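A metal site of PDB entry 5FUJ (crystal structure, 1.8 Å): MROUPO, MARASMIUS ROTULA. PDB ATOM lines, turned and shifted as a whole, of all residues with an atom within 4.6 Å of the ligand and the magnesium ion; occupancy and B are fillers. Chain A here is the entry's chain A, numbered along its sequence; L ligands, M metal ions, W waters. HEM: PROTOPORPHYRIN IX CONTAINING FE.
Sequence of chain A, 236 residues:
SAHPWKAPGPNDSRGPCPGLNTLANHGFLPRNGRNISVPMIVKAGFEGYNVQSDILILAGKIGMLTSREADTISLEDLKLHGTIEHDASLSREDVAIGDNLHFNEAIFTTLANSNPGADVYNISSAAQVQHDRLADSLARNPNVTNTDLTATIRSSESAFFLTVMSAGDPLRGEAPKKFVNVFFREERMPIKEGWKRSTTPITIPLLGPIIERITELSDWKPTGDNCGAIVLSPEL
Within 4 Å of the magnesium ion: Glu 85, His 86 and Ser 89.
Merely in contact with the ligand: Pro 16 (3.7 Å), Pro 18 (3.6 Å), Gly 19 (3.6 Å), Leu 20 (3.7 Å), Ile 41 (3.8 Å), Tyr 49 (3.8 Å), Leu 56 (3.8 Å), Ala 59 (3.7 Å), Gly 60 (3.7 Å), Leu 78 (3.4 Å), Ile 84 (3.4 Å), Arg 92 (3.9 Å), Glu 157 (3.4 Å), Phe 160 (3.6 Å) and Phe 184 (3.9 Å).
Of the 29 residues printed, 21 come within 4 Å of the ligand.
The nearest printed residue that does not touch the ligand is Val 164 (4.02 Å).
Water W3 is bound to the magnesium ion (2.1 Å).
The magnesium ion is bound by water W4 (2.1 Å).
OE2 of Glu 85 is bound to the magnesium ion, at 2.2 Å.
The magnesium ion is bound by O1D of the ligand, at 2.2 Å.
The magnesium ion is bound by OG of Ser 89, 2.2 Å away.
The magnesium ion is bound by the backbone carbonyl oxygen (O) of His 86, at 2.2 Å.
OE1 of Glu 85 lies within hydrogen-bond range of ND2 of Asn 100, at 3.1 Å.
NE2 of His 86 is in hydrogen-bond range of OE1 of Glu 157, 2.6 Å away.
SG of Cys 17 lies close to N of Gly 19.
SG of Cys 17 sits close to N of Leu 20.
The side-chain hydroxyl (OG) of Ser 91 sits at hydrogen-bond distance from the guanidinium group (NH1) of Arg 92, 2.8 Å away.
O of Gly 19 sits at hydrogen-bond distance from OH of Tyr 49.
Water W2 bridges an oxygen (O2A) of the ligand (2.7 Å) and the side-chain carboxylate of Glu 157 (2.8 Å).
Water W1 bridges O of Pro 16 (2.8 Å) and O2D of the ligand (2.9 Å).
The backbone NH (N) of His 86 lies close to an oxygen (O1D) of the ligand.
O2D of the ligand lies close to NE2 of His 86 (3.4 Å).
An iron atom (FE) of the ligand is bound by the side-chain sulfur (SG) of Cys 17, at 2.3 Å.
The backbone NH of Ser 91 sits at hydrogen-bond distance from an oxygen (O1A) of the ligand (2.8 Å).
O1A of the ligand is in hydrogen-bond range of OG of Ser 91 (2.7 Å).
An oxygen (O2A) of the ligand lies within hydrogen-bond range of the backbone NH (N) of Leu 90, 2.7 Å away.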
ATOM      1  N   PRO A  16       2.356 -32.136   4.209  1.00  0.00           N
ATOM      2  CA  PRO A  16       2.609 -32.044   2.767  1.00  0.00           C
ATOM      3  C   PRO A  16       1.783 -30.978   2.060  1.00  0.00           C
ATOM      4  O   PRO A  16       1.888 -30.843   0.821  1.00  0.00           O
ATOM      5  CB  PRO A  16       2.216 -33.441   2.283  1.00  0.00           C
ATOM      6  CG  PRO A  16       1.052 -33.792   3.190  1.00  0.00           C
ATOM      7  CD  PRO A  16       1.489 -33.278   4.558  1.00  0.00           C
ATOM      8  N   CYS A  17       0.923 -30.289   2.815  1.00  0.00           N
ATOM      9  CA  CYS A  17      -0.003 -29.276   2.233  1.00  0.00           C
ATOM     10  C   CYS A  17       0.492 -27.855   2.461  1.00  0.00           C
ATOM     11  O   CYS A  17       0.435 -27.335   3.570  1.00  0.00           O
ATOM     12  CB  CYS A  17      -1.407 -29.420   2.840  1.00  0.00           C
ATOM     13  SG  CYS A  17      -2.578 -28.187   2.220  1.00  0.00           S
ATOM     14  N   PRO A  18       0.845 -27.151   1.380  1.00  0.00           N
ATOM     15  CA  PRO A  18       1.209 -25.762   1.555  1.00  0.00           C
ATOM     16  C   PRO A  18       0.057 -24.888   2.047  1.00  0.00           C
ATOM     17  O   PRO A  18       0.287 -23.845   2.664  1.00  0.00           O
ATOM     18  CB  PRO A  18       1.654 -25.323   0.155  1.00  0.00           C
ATOM     19  CG  PRO A  18       0.907 -26.243  -0.783  1.00  0.00           C
ATOM     20  CD  PRO A  18       0.840 -27.563  -0.045  1.00  0.00           C
ATOM     21  N   GLY A  19      -1.176 -25.217   1.654  1.00  0.00           N
ATOM     22  CA  GLY A  19      -2.327 -24.396   2.097  1.00  0.00           C
ATOM     23  C   GLY A  19      -2.444 -24.359   3.634  1.00  0.00           C
ATOM     24  O   GLY A  19      -2.507 -23.283   4.237  1.00  0.00           O
ATOM     25  N   LEU A  20      -2.443 -25.537   4.253  1.00  0.00           N
ATOM     26  CA  LEU A  20      -2.575 -25.628   5.717  1.00  0.00           C
ATOM     27  C   LEU A  20      -1.274 -25.192   6.410  1.00  0.00           C
ATOM     28  O   LEU A  20      -1.312 -24.482   7.417  1.00  0.00           O
ATOM     29  CB  LEU A  20      -2.885 -27.072   6.143  1.00  0.00           C
ATOM     30  CG  LEU A  20      -4.228 -27.624   5.634  1.00  0.00           C
ATOM     31  CD1 LEU A  20      -4.416 -29.010   6.192  1.00  0.00           C
ATOM     32  CD2 LEU A  20      -5.406 -26.750   6.085  1.00  0.00           C
ATOM     33  N   LEU A  23      -1.298 -21.443   6.607  1.00  0.00           N
ATOM     34  CA  LEU A  23      -2.189 -20.920   7.626  1.00  0.00           C
ATOM     35  C   LEU A  23      -1.557 -21.066   9.035  1.00  0.00           C
ATOM     36  O   LEU A  23      -1.743 -20.175   9.862  1.00  0.00           O
ATOM     37  CB  LEU A  23      -3.574 -21.588   7.605  1.00  0.00           C
ATOM     38  CG  LEU A  23      -4.375 -21.313   6.326  1.00  0.00           C
ATOM     39  CD1 LEU A  23      -5.566 -22.295   6.234  1.00  0.00           C
ATOM     40  CD2 LEU A  23      -4.834 -19.868   6.179  1.00  0.00           C
ATOM     41  N   ILE A  41      -9.943 -25.816  10.859  1.00  0.00           N
ATOM     42  CA  ILE A  41      -9.627 -25.687   9.435  1.00  0.00           C
ATOM     43  C   ILE A  41     -10.627 -24.825   8.667  1.00  0.00           C
ATOM     44  O   ILE A  41     -10.247 -23.959   7.874  1.00  0.00           O
ATOM     45  CB  ILE A  41      -9.506 -27.083   8.779  1.00  0.00           C
ATOM     46  CG1 ILE A  41      -8.263 -27.825   9.305  1.00  0.00           C
ATOM     47  CG2 ILE A  41      -9.460 -26.933   7.235  1.00  0.00           C
ATOM     48  CD1 ILE A  41      -8.229 -29.312   8.924  1.00  0.00           C
ATOM     49  N   GLY A  45      -9.290 -21.397   6.986  1.00  0.00           N
ATOM     50  CA  GLY A  45      -9.314 -21.304   5.538  1.00  0.00           C
ATOM     51  C   GLY A  45     -10.244 -20.196   5.089  1.00  0.00           C
ATOM     52  O   GLY A  45      -9.961 -19.503   4.105  1.00  0.00           O
ATOM     53  N   TYR A  49      -8.094 -17.199   3.387  1.00  0.00           N
ATOM     54  CA  TYR A  49      -8.107 -17.361   1.916  1.00  0.00           C
ATOM     55  C   TYR A  49      -9.498 -17.084   1.314  1.00  0.00           C
ATOM     56  O   TYR A  49      -9.651 -17.095   0.090  1.00  0.00           O
ATOM     57  CB  TYR A  49      -7.733 -18.798   1.549  1.00  0.00           C
ATOM     58  CG  TYR A  49      -6.393 -19.297   2.026  1.00  0.00           C
ATOM     59  CD1 TYR A  49      -5.251 -18.483   1.960  1.00  0.00           C
ATOM     60  CD2 TYR A  49      -6.238 -20.634   2.370  1.00  0.00           C
ATOM     61  CE1 TYR A  49      -4.009 -18.998   2.286  1.00  0.00           C
ATOM     62  CE2 TYR A  49      -5.001 -21.150   2.704  1.00  0.00           C
ATOM     63  CZ  TYR A  49      -3.882 -20.314   2.672  1.00  0.00           C
ATOM     64  OH  TYR A  49      -2.643 -20.869   2.947  1.00  0.00           O
ATOM     65  N   LEU A  56     -13.837 -27.402   2.629  1.00  0.00           N
ATOM     66  CA  LEU A  56     -13.009 -27.617   3.819  1.00  0.00           C
ATOM     67  C   LEU A  56     -13.543 -28.697   4.755  1.00  0.00           C
ATOM     68  O   LEU A  56     -12.759 -29.436   5.394  1.00  0.00           O
ATOM     69  CB  LEU A  56     -12.754 -26.307   4.557  1.00  0.00           C
ATOM     70  CG  LEU A  56     -11.960 -25.300   3.709  1.00  0.00           C
ATOM     71  CD1 LEU A  56     -11.779 -23.982   4.445  1.00  0.00           C
ATOM     72  CD2 LEU A  56     -10.588 -25.873   3.337  1.00  0.00           C
ATOM     73  N   ALA A  59     -12.812 -32.092   2.597  1.00  0.00           N
ATOM     74  CA  ALA A  59     -11.404 -32.471   2.652  1.00  0.00           C
ATOM     75  C   ALA A  59     -10.953 -32.718   4.082  1.00  0.00           C
ATOM     76  O   ALA A  59     -10.196 -33.647   4.347  1.00  0.00           O
ATOM     77  CB  ALA A  59     -10.537 -31.395   2.000  1.00  0.00           C
ATOM     78  N   GLY A  60     -11.406 -31.847   4.994  1.00  0.00           N
ATOM     79  CA  GLY A  60     -11.000 -31.938   6.410  1.00  0.00           C
ATOM     80  C   GLY A  60     -11.344 -33.243   7.095  1.00  0.00           C
ATOM     81  O   GLY A  60     -10.513 -33.839   7.793  1.00  0.00           O
ATOM     82  N   GLY A  63      -9.064 -35.886   5.926  1.00  0.00           N
ATOM     83  CA  GLY A  63      -7.762 -35.677   6.553  1.00  0.00           C
ATOM     84  C   GLY A  63      -7.712 -36.159   7.996  1.00  0.00           C
ATOM     85  O   GLY A  63      -6.658 -36.626   8.450  1.00  0.00           O
ATOM     86  N   LEU A  78      -0.841 -35.747   7.889  1.00  0.00           N
ATOM     87  CA  LEU A  78      -1.458 -35.724   6.571  1.00  0.00           C
ATOM     88  C   LEU A  78      -0.551 -36.331   5.512  1.00  0.00           C
ATOM     89  O   LEU A  78      -0.983 -36.554   4.360  1.00  0.00           O
ATOM     90  CB  LEU A  78      -1.839 -34.295   6.186  1.00  0.00           C
ATOM     91  CG  LEU A  78      -3.059 -33.754   6.948  1.00  0.00           C
ATOM     92  CD1 LEU A  78      -3.181 -32.262   6.715  1.00  0.00           C
ATOM     93  CD2 LEU A  78      -4.355 -34.492   6.587  1.00  0.00           C
ATOM     94  N   ILE A  84      -5.087 -38.899   1.608  1.00  0.00           N
ATOM     95  CA  ILE A  84      -5.043 -37.816   0.608  1.00  0.00           C
ATOM     96  C   ILE A  84      -3.671 -37.743  -0.095  1.00  0.00           C
ATOM     97  O   ILE A  84      -3.588 -37.612  -1.325  1.00  0.00           O
ATOM     98  CB  ILE A  84      -5.379 -36.450   1.240  1.00  0.00           C
ATOM     99  CG1 ILE A  84      -6.819 -36.462   1.754  1.00  0.00           C
ATOM    100  CG2 ILE A  84      -5.200 -35.315   0.223  1.00  0.00           C
ATOM    101  CD1 ILE A  84      -7.095 -35.321   2.721  1.00  0.00           C
ATOM    102  N   GLU A  85      -2.604 -38.000   0.652  1.00  0.00           N
ATOM    103  CA  GLU A  85      -1.265 -37.787   0.087  1.00  0.00           C
ATOM    104  C   GLU A  85      -1.073 -38.788  -1.053  1.00  0.00           C
ATOM    105  O   GLU A  85      -1.476 -39.932  -0.947  1.00  0.00           O
ATOM    106  CB  GLU A  85      -0.188 -37.965   1.155  1.00  0.00           C
ATOM    107  CG  GLU A  85       1.215 -37.520   0.701  1.00  0.00           C
ATOM    108  CD  GLU A  85       1.887 -38.545  -0.214  1.00  0.00           C
ATOM    109  OE1 GLU A  85       1.705 -39.755   0.004  1.00  0.00           O
ATOM    110  OE2 GLU A  85       2.556 -38.137  -1.212  1.00  0.00           O
ATOM    111  N   HIS A  86      -0.454 -38.343  -2.144  1.00  0.00           N
ATOM    112  CA  HIS A  86      -0.423 -39.112  -3.398  1.00  0.00           C
ATOM    113  C   HIS A  86       0.902 -38.896  -4.104  1.00  0.00           C
ATOM    114  O   HIS A  86       1.567 -37.865  -3.918  1.00  0.00           O
ATOM    115  CB  HIS A  86      -1.580 -38.651  -4.331  1.00  0.00           C
ATOM    116  CG  HIS A  86      -1.604 -37.167  -4.559  1.00  0.00           C
ATOM    117  ND1 HIS A  86      -0.665 -36.508  -5.332  1.00  0.00           N
ATOM    118  CD2 HIS A  86      -2.408 -36.204  -4.048  1.00  0.00           C
ATOM    119  CE1 HIS A  86      -0.905 -35.215  -5.300  1.00  0.00           C
ATOM    120  NE2 HIS A  86      -1.951 -35.007  -4.515  1.00  0.00           N
ATOM    121  N   ASP A  87       1.214 -39.796  -5.028  1.00  0.00           N
ATOM    122  CA  ASP A  87       2.322 -39.616  -5.965  1.00  0.00           C
ATOM    123  C   ASP A  87       2.097 -38.491  -6.965  1.00  0.00           C
ATOM    124  O   ASP A  87       0.966 -37.982  -7.121  1.00  0.00           O
ATOM    125  CB  ASP A  87       2.586 -40.954  -6.705  1.00  0.00           C
ATOM    126  CG  ASP A  87       2.860 -42.108  -5.746  1.00  0.00           C
ATOM    127  OD1 ASP A  87       3.441 -41.868  -4.662  1.00  0.00           O
ATOM    128  OD2 ASP A  87       2.437 -43.245  -6.050  1.00  0.00           O
ATOM    129  N   SER A  89       3.063 -35.358  -6.819  1.00  0.00           N
ATOM    130  CA  SER A  89       2.921 -34.028  -6.251  1.00  0.00           C
ATOM    131  C   SER A  89       3.725 -33.005  -7.019  1.00  0.00           C
ATOM    132  O   SER A  89       4.702 -33.336  -7.710  1.00  0.00           O
ATOM    133  CB  SER A  89       3.357 -34.026  -4.776  1.00  0.00           C
ATOM    134  OG  SER A  89       2.513 -34.870  -4.030  1.00  0.00           O
ATOM    135  N   LEU A  90       3.319 -31.757  -6.836  1.00  0.00           N
ATOM    136  CA  LEU A  90       3.925 -30.631  -7.494  1.00  0.00           C
ATOM    137  C   LEU A  90       5.243 -30.243  -6.850  1.00  0.00           C
ATOM    138  O   LEU A  90       6.019 -29.541  -7.478  1.00  0.00           O
ATOM    139  CB  LEU A  90       2.999 -29.416  -7.443  1.00  0.00           C
ATOM    140  CG  LEU A  90       1.604 -29.613  -8.061  1.00  0.00           C
ATOM    141  CD1 LEU A  90       0.688 -28.494  -7.585  1.00  0.00           C
ATOM    142  CD2 LEU A  90       1.743 -29.597  -9.582  1.00  0.00           C
ATOM    143  N   SER A  91       5.436 -30.577  -5.573  1.00  0.00           N
ATOM    144  CA  SER A  91       6.554 -29.974  -4.817  1.00  0.00           C
ATOM    145  C   SER A  91       7.142 -30.911  -3.773  1.00  0.00           C
ATOM    146  O   SER A  91       8.043 -30.503  -3.047  1.00  0.00           O
ATOM    147  CB  SER A  91       6.140 -28.646  -4.142  1.00  0.00           C
ATOM    148  OG  SER A  91       5.316 -28.889  -3.003  1.00  0.00           O
ATOM    149  N   ARG A  92       6.676 -32.162  -3.748  1.00  0.00           N
ATOM    150  CA  ARG A  92       7.184 -33.221  -2.857  1.00  0.00           C
ATOM    151  C   ARG A  92       7.573 -34.444  -3.703  1.00  0.00           C
ATOM    152  O   ARG A  92       7.027 -34.638  -4.798  1.00  0.00           O
ATOM    153  CB  ARG A  92       6.097 -33.636  -1.839  1.00  0.00           C
ATOM    154  CG  ARG A  92       6.123 -32.849  -0.534  1.00  0.00           C
ATOM    155  CD  ARG A  92       5.836 -31.379  -0.698  1.00  0.00           C
ATOM    156  NE  ARG A  92       5.637 -30.766   0.631  1.00  0.00           N
ATOM    157  CZ  ARG A  92       5.433 -29.471   0.832  1.00  0.00           C
ATOM    158  NH1 ARG A  92       5.428 -28.638  -0.197  1.00  0.00           N
ATOM    159  NH2 ARG A  92       5.310 -28.990   2.088  1.00  0.00           N
ATOM    160  N   ASN A 100       7.984 -37.667   0.956  1.00  0.00           N
ATOM    161  CA  ASN A 100       6.626 -37.197   0.562  1.00  0.00           C
ATOM    162  C   ASN A 100       6.077 -36.066   1.406  1.00  0.00           C
ATOM    163  O   ASN A 100       4.920 -35.655   1.242  1.00  0.00           O
ATOM    164  CB  ASN A 100       5.626 -38.374   0.532  1.00  0.00           C
ATOM    165  CG  ASN A 100       5.193 -38.835   1.915  1.00  0.00           C
ATOM    166  OD1 ASN A 100       5.829 -38.486   2.931  1.00  0.00           O
ATOM    167  ND2 ASN A 100       4.074 -39.581   1.986  1.00  0.00           N
ATOM    168  N   GLU A 157      -5.911 -29.663  -6.196  1.00  0.00           N
ATOM    169  CA  GLU A 157      -4.780 -28.923  -5.620  1.00  0.00           C
ATOM    170  C   GLU A 157      -4.221 -27.838  -6.528  1.00  0.00           C
ATOM    171  O   GLU A 157      -3.947 -26.724  -6.059  1.00  0.00           O
ATOM    172  CB  GLU A 157      -3.704 -29.901  -5.093  1.00  0.00           C
ATOM    173  CG  GLU A 157      -4.251 -30.686  -3.891  1.00  0.00           C
ATOM    174  CD  GLU A 157      -3.576 -32.024  -3.608  1.00  0.00           C
ATOM    175  OE1 GLU A 157      -2.746 -32.493  -4.424  1.00  0.00           O
ATOM    176  OE2 GLU A 157      -3.948 -32.673  -2.611  1.00  0.00           O
ATOM    177  N   PHE A 160      -6.656 -25.170  -6.402  1.00  0.00           N
ATOM    178  CA  PHE A 160      -6.481 -24.429  -5.143  1.00  0.00           C
ATOM    179  C   PHE A 160      -5.412 -23.329  -5.286  1.00  0.00           C
ATOM    180  O   PHE A 160      -5.634 -22.194  -4.897  1.00  0.00           O
ATOM    181  CB  PHE A 160      -6.130 -25.376  -3.970  1.00  0.00           C
ATOM    182  CG  PHE A 160      -7.263 -25.598  -3.013  1.00  0.00           C
ATOM    183  CD1 PHE A 160      -8.171 -24.578  -2.740  1.00  0.00           C
ATOM    184  CD2 PHE A 160      -7.358 -26.780  -2.291  1.00  0.00           C
ATOM    185  CE1 PHE A 160      -9.180 -24.753  -1.808  1.00  0.00           C
ATOM    186  CE2 PHE A 160      -8.401 -26.986  -1.395  1.00  0.00           C
ATOM    187  CZ  PHE A 160      -9.291 -25.948  -1.133  1.00  0.00           C
ATOM    188  N   PHE A 161      -4.229 -23.678  -5.778  1.00  0.00           N
ATOM    189  CA  PHE A 161      -3.163 -22.655  -5.804  1.00  0.00           C
ATOM    190  C   PHE A 161      -3.457 -21.576  -6.863  1.00  0.00           C
ATOM    191  O   PHE A 161      -3.209 -20.382  -6.627  1.00  0.00           O
ATOM    192  CB  PHE A 161      -1.741 -23.259  -5.914  1.00  0.00           C
ATOM    193  CG  PHE A 161      -1.291 -23.558  -7.319  1.00  0.00           C
ATOM    194  CD1 PHE A 161      -1.057 -22.518  -8.241  1.00  0.00           C
ATOM    195  CD2 PHE A 161      -1.069 -24.867  -7.725  1.00  0.00           C
ATOM    196  CE1 PHE A 161      -0.637 -22.797  -9.522  1.00  0.00           C
ATOM    197  CE2 PHE A 161      -0.640 -25.160  -9.011  1.00  0.00           C
ATOM    198  CZ  PHE A 161      -0.419 -24.111  -9.906  1.00  0.00           C
ATOM    199  N   VAL A 164      -6.570 -19.498  -4.812  1.00  0.00           N
ATOM    200  CA  VAL A 164      -6.254 -18.868  -3.521  1.00  0.00           C
ATOM    201  C   VAL A 164      -5.127 -17.802  -3.662  1.00  0.00           C
ATOM    202  O   VAL A 164      -5.160 -16.737  -2.992  1.00  0.00           O
ATOM    203  CB  VAL A 164      -5.913 -19.929  -2.478  1.00  0.00           C
ATOM    204  CG1 VAL A 164      -5.289 -19.329  -1.235  1.00  0.00           C
ATOM    205  CG2 VAL A 164      -7.177 -20.705  -2.109  1.00  0.00           C
ATOM    206  N   PHE A 183       4.255 -18.819  -1.929  1.00  0.00           N
ATOM    207  CA  PHE A 183       3.350 -19.805  -1.299  1.00  0.00           C
ATOM    208  C   PHE A 183       3.992 -21.190  -1.111  1.00  0.00           C
ATOM    209  O   PHE A 183       3.962 -21.739  -0.014  1.00  0.00           O
ATOM    210  CB  PHE A 183       2.065 -19.898  -2.153  1.00  0.00           C
ATOM    211  CG  PHE A 183       1.008 -20.831  -1.612  1.00  0.00           C
ATOM    212  CD1 PHE A 183       0.284 -20.514  -0.463  1.00  0.00           C
ATOM    213  CD2 PHE A 183       0.653 -21.973  -2.329  1.00  0.00           C
ATOM    214  CE1 PHE A 183      -0.712 -21.378  -0.012  1.00  0.00           C
ATOM    215  CE2 PHE A 183      -0.378 -22.788  -1.923  1.00  0.00           C
ATOM    216  CZ  PHE A 183      -1.061 -22.506  -0.748  1.00  0.00           C
ATOM    217  N   PHE A 184       4.516 -21.785  -2.185  1.00  0.00           N
ATOM    218  CA  PHE A 184       5.161 -23.114  -2.114  1.00  0.00           C
ATOM    219  C   PHE A 184       6.505 -23.095  -1.355  1.00  0.00           C
ATOM    220  O   PHE A 184       6.722 -23.909  -0.449  1.00  0.00           O
ATOM    221  CB  PHE A 184       5.385 -23.694  -3.511  1.00  0.00           C
ATOM    222  CG  PHE A 184       4.183 -24.417  -4.085  1.00  0.00           C
ATOM    223  CD1 PHE A 184       3.969 -25.758  -3.833  1.00  0.00           C
ATOM    224  CD2 PHE A 184       3.266 -23.719  -4.863  1.00  0.00           C
ATOM    225  CE1 PHE A 184       2.859 -26.418  -4.368  1.00  0.00           C
ATOM    226  CE2 PHE A 184       2.169 -24.360  -5.402  1.00  0.00           C
ATOM    227  CZ  PHE A 184       1.975 -25.714  -5.172  1.00  0.00           C
HETATM  228  CHA HEM L   1      -1.563 -30.816  -0.980  1.00  0.00           C
HETATM  229  CHB HEM L   1      -3.421 -26.333  -1.271  1.00  0.00           C
HETATM  230  CHC HEM L   1      -6.566 -27.518   2.330  1.00  0.00           C
HETATM  231  CHD HEM L   1      -4.519 -31.915   2.716  1.00  0.00           C
HETATM  232  C1A HEM L   1      -1.902 -29.565  -1.426  1.00  0.00           C
HETATM  233  C2A HEM L   1      -1.307 -28.941  -2.563  1.00  0.00           C
HETATM  234  C3A HEM L   1      -1.823 -27.689  -2.657  1.00  0.00           C
HETATM  235  C4A HEM L   1      -2.733 -27.512  -1.577  1.00  0.00           C
HETATM  236  CMA HEM L   1      -1.487 -26.668  -3.729  1.00  0.00           C
HETATM  237  CAA HEM L   1      -0.341 -29.611  -3.523  1.00  0.00           C
HETATM  238  CBA HEM L   1       1.090 -29.739  -2.951  1.00  0.00           C
HETATM  239  CGA HEM L   1       1.969 -30.473  -3.959  1.00  0.00           C
HETATM  240  O1A HEM L   1       3.221 -30.381  -3.850  1.00  0.00           O
HETATM  241  O2A HEM L   1       1.471 -31.152  -4.915  1.00  0.00           O
HETATM  242  C1B HEM L   1      -4.407 -26.277  -0.245  1.00  0.00           C
HETATM  243  C2B HEM L   1      -5.158 -25.090   0.042  1.00  0.00           C
HETATM  244  C3B HEM L   1      -6.004 -25.380   1.069  1.00  0.00           C
HETATM  245  C4B HEM L   1      -5.792 -26.792   1.401  1.00  0.00           C
HETATM  246  CMB HEM L   1      -4.997 -23.725  -0.595  1.00  0.00           C
HETATM  247  CAB HEM L   1      -6.969 -24.425   1.676  1.00  0.00           C
HETATM  248  CBB HEM L   1      -7.081 -24.353   3.013  1.00  0.00           C
HETATM  249  C1C HEM L   1      -6.374 -28.863   2.651  1.00  0.00           C
HETATM  250  C2C HEM L   1      -7.148 -29.589   3.581  1.00  0.00           C
HETATM  251  C3C HEM L   1      -6.549 -30.831   3.720  1.00  0.00           C
HETATM  252  C4C HEM L   1      -5.390 -30.856   2.847  1.00  0.00           C
HETATM  253  CMC HEM L   1      -8.385 -29.020   4.272  1.00  0.00           C
HETATM  254  CAC HEM L   1      -6.958 -31.962   4.582  1.00  0.00           C
HETATM  255  CBC HEM L   1      -7.301 -31.721   5.853  1.00  0.00           C
HETATM  256  C1D HEM L   1      -3.545 -31.904   1.708  1.00  0.00           C
HETATM  257  C2D HEM L   1      -2.631 -33.051   1.555  1.00  0.00           C
HETATM  258  C3D HEM L   1      -1.855 -32.771   0.505  1.00  0.00           C
HETATM  259  C4D HEM L   1      -2.230 -31.413   0.086  1.00  0.00           C
HETATM  260  CMD HEM L   1      -2.666 -34.350   2.326  1.00  0.00           C
HETATM  261  CAD HEM L   1      -0.765 -33.671  -0.040  1.00  0.00           C
HETATM  262  CBD HEM L   1      -1.203 -34.225  -1.423  1.00  0.00           C
HETATM  263  CGD HEM L   1       0.089 -34.514  -2.190  1.00  0.00           C
HETATM  264  O1D HEM L   1       0.548 -35.654  -2.130  1.00  0.00           O
HETATM  265  O2D HEM L   1       0.662 -33.638  -2.901  1.00  0.00           O
HETATM  266  NA  HEM L   1      -2.777 -28.694  -0.808  1.00  0.00           N
HETATM  267  NB  HEM L   1      -4.820 -27.273   0.582  1.00  0.00           N
HETATM  268  NC  HEM L   1      -5.314 -29.654   2.232  1.00  0.00           N
HETATM  269  ND  HEM L   1      -3.268 -30.922   0.812  1.00  0.00           N
HETATM  270 FE   HEM L   1      -4.005 -29.173   0.691  1.00  0.00          FE
HETATM  271 MG    MG M   1       2.512 -36.458  -2.556  1.00  0.00          MG
HETATM  272  O   HOH W   1       2.707 -32.619  -1.185  1.00  0.00           O
HETATM  273  O   HOH W   2      -0.683 -32.090  -6.269  1.00  0.00           O
HETATM  274  O   HOH W   3       4.393 -37.035  -3.260  1.00  0.00           O
HETATM  275  O   HOH W   4       3.224 -35.210  -0.982  1.00  0.00           O
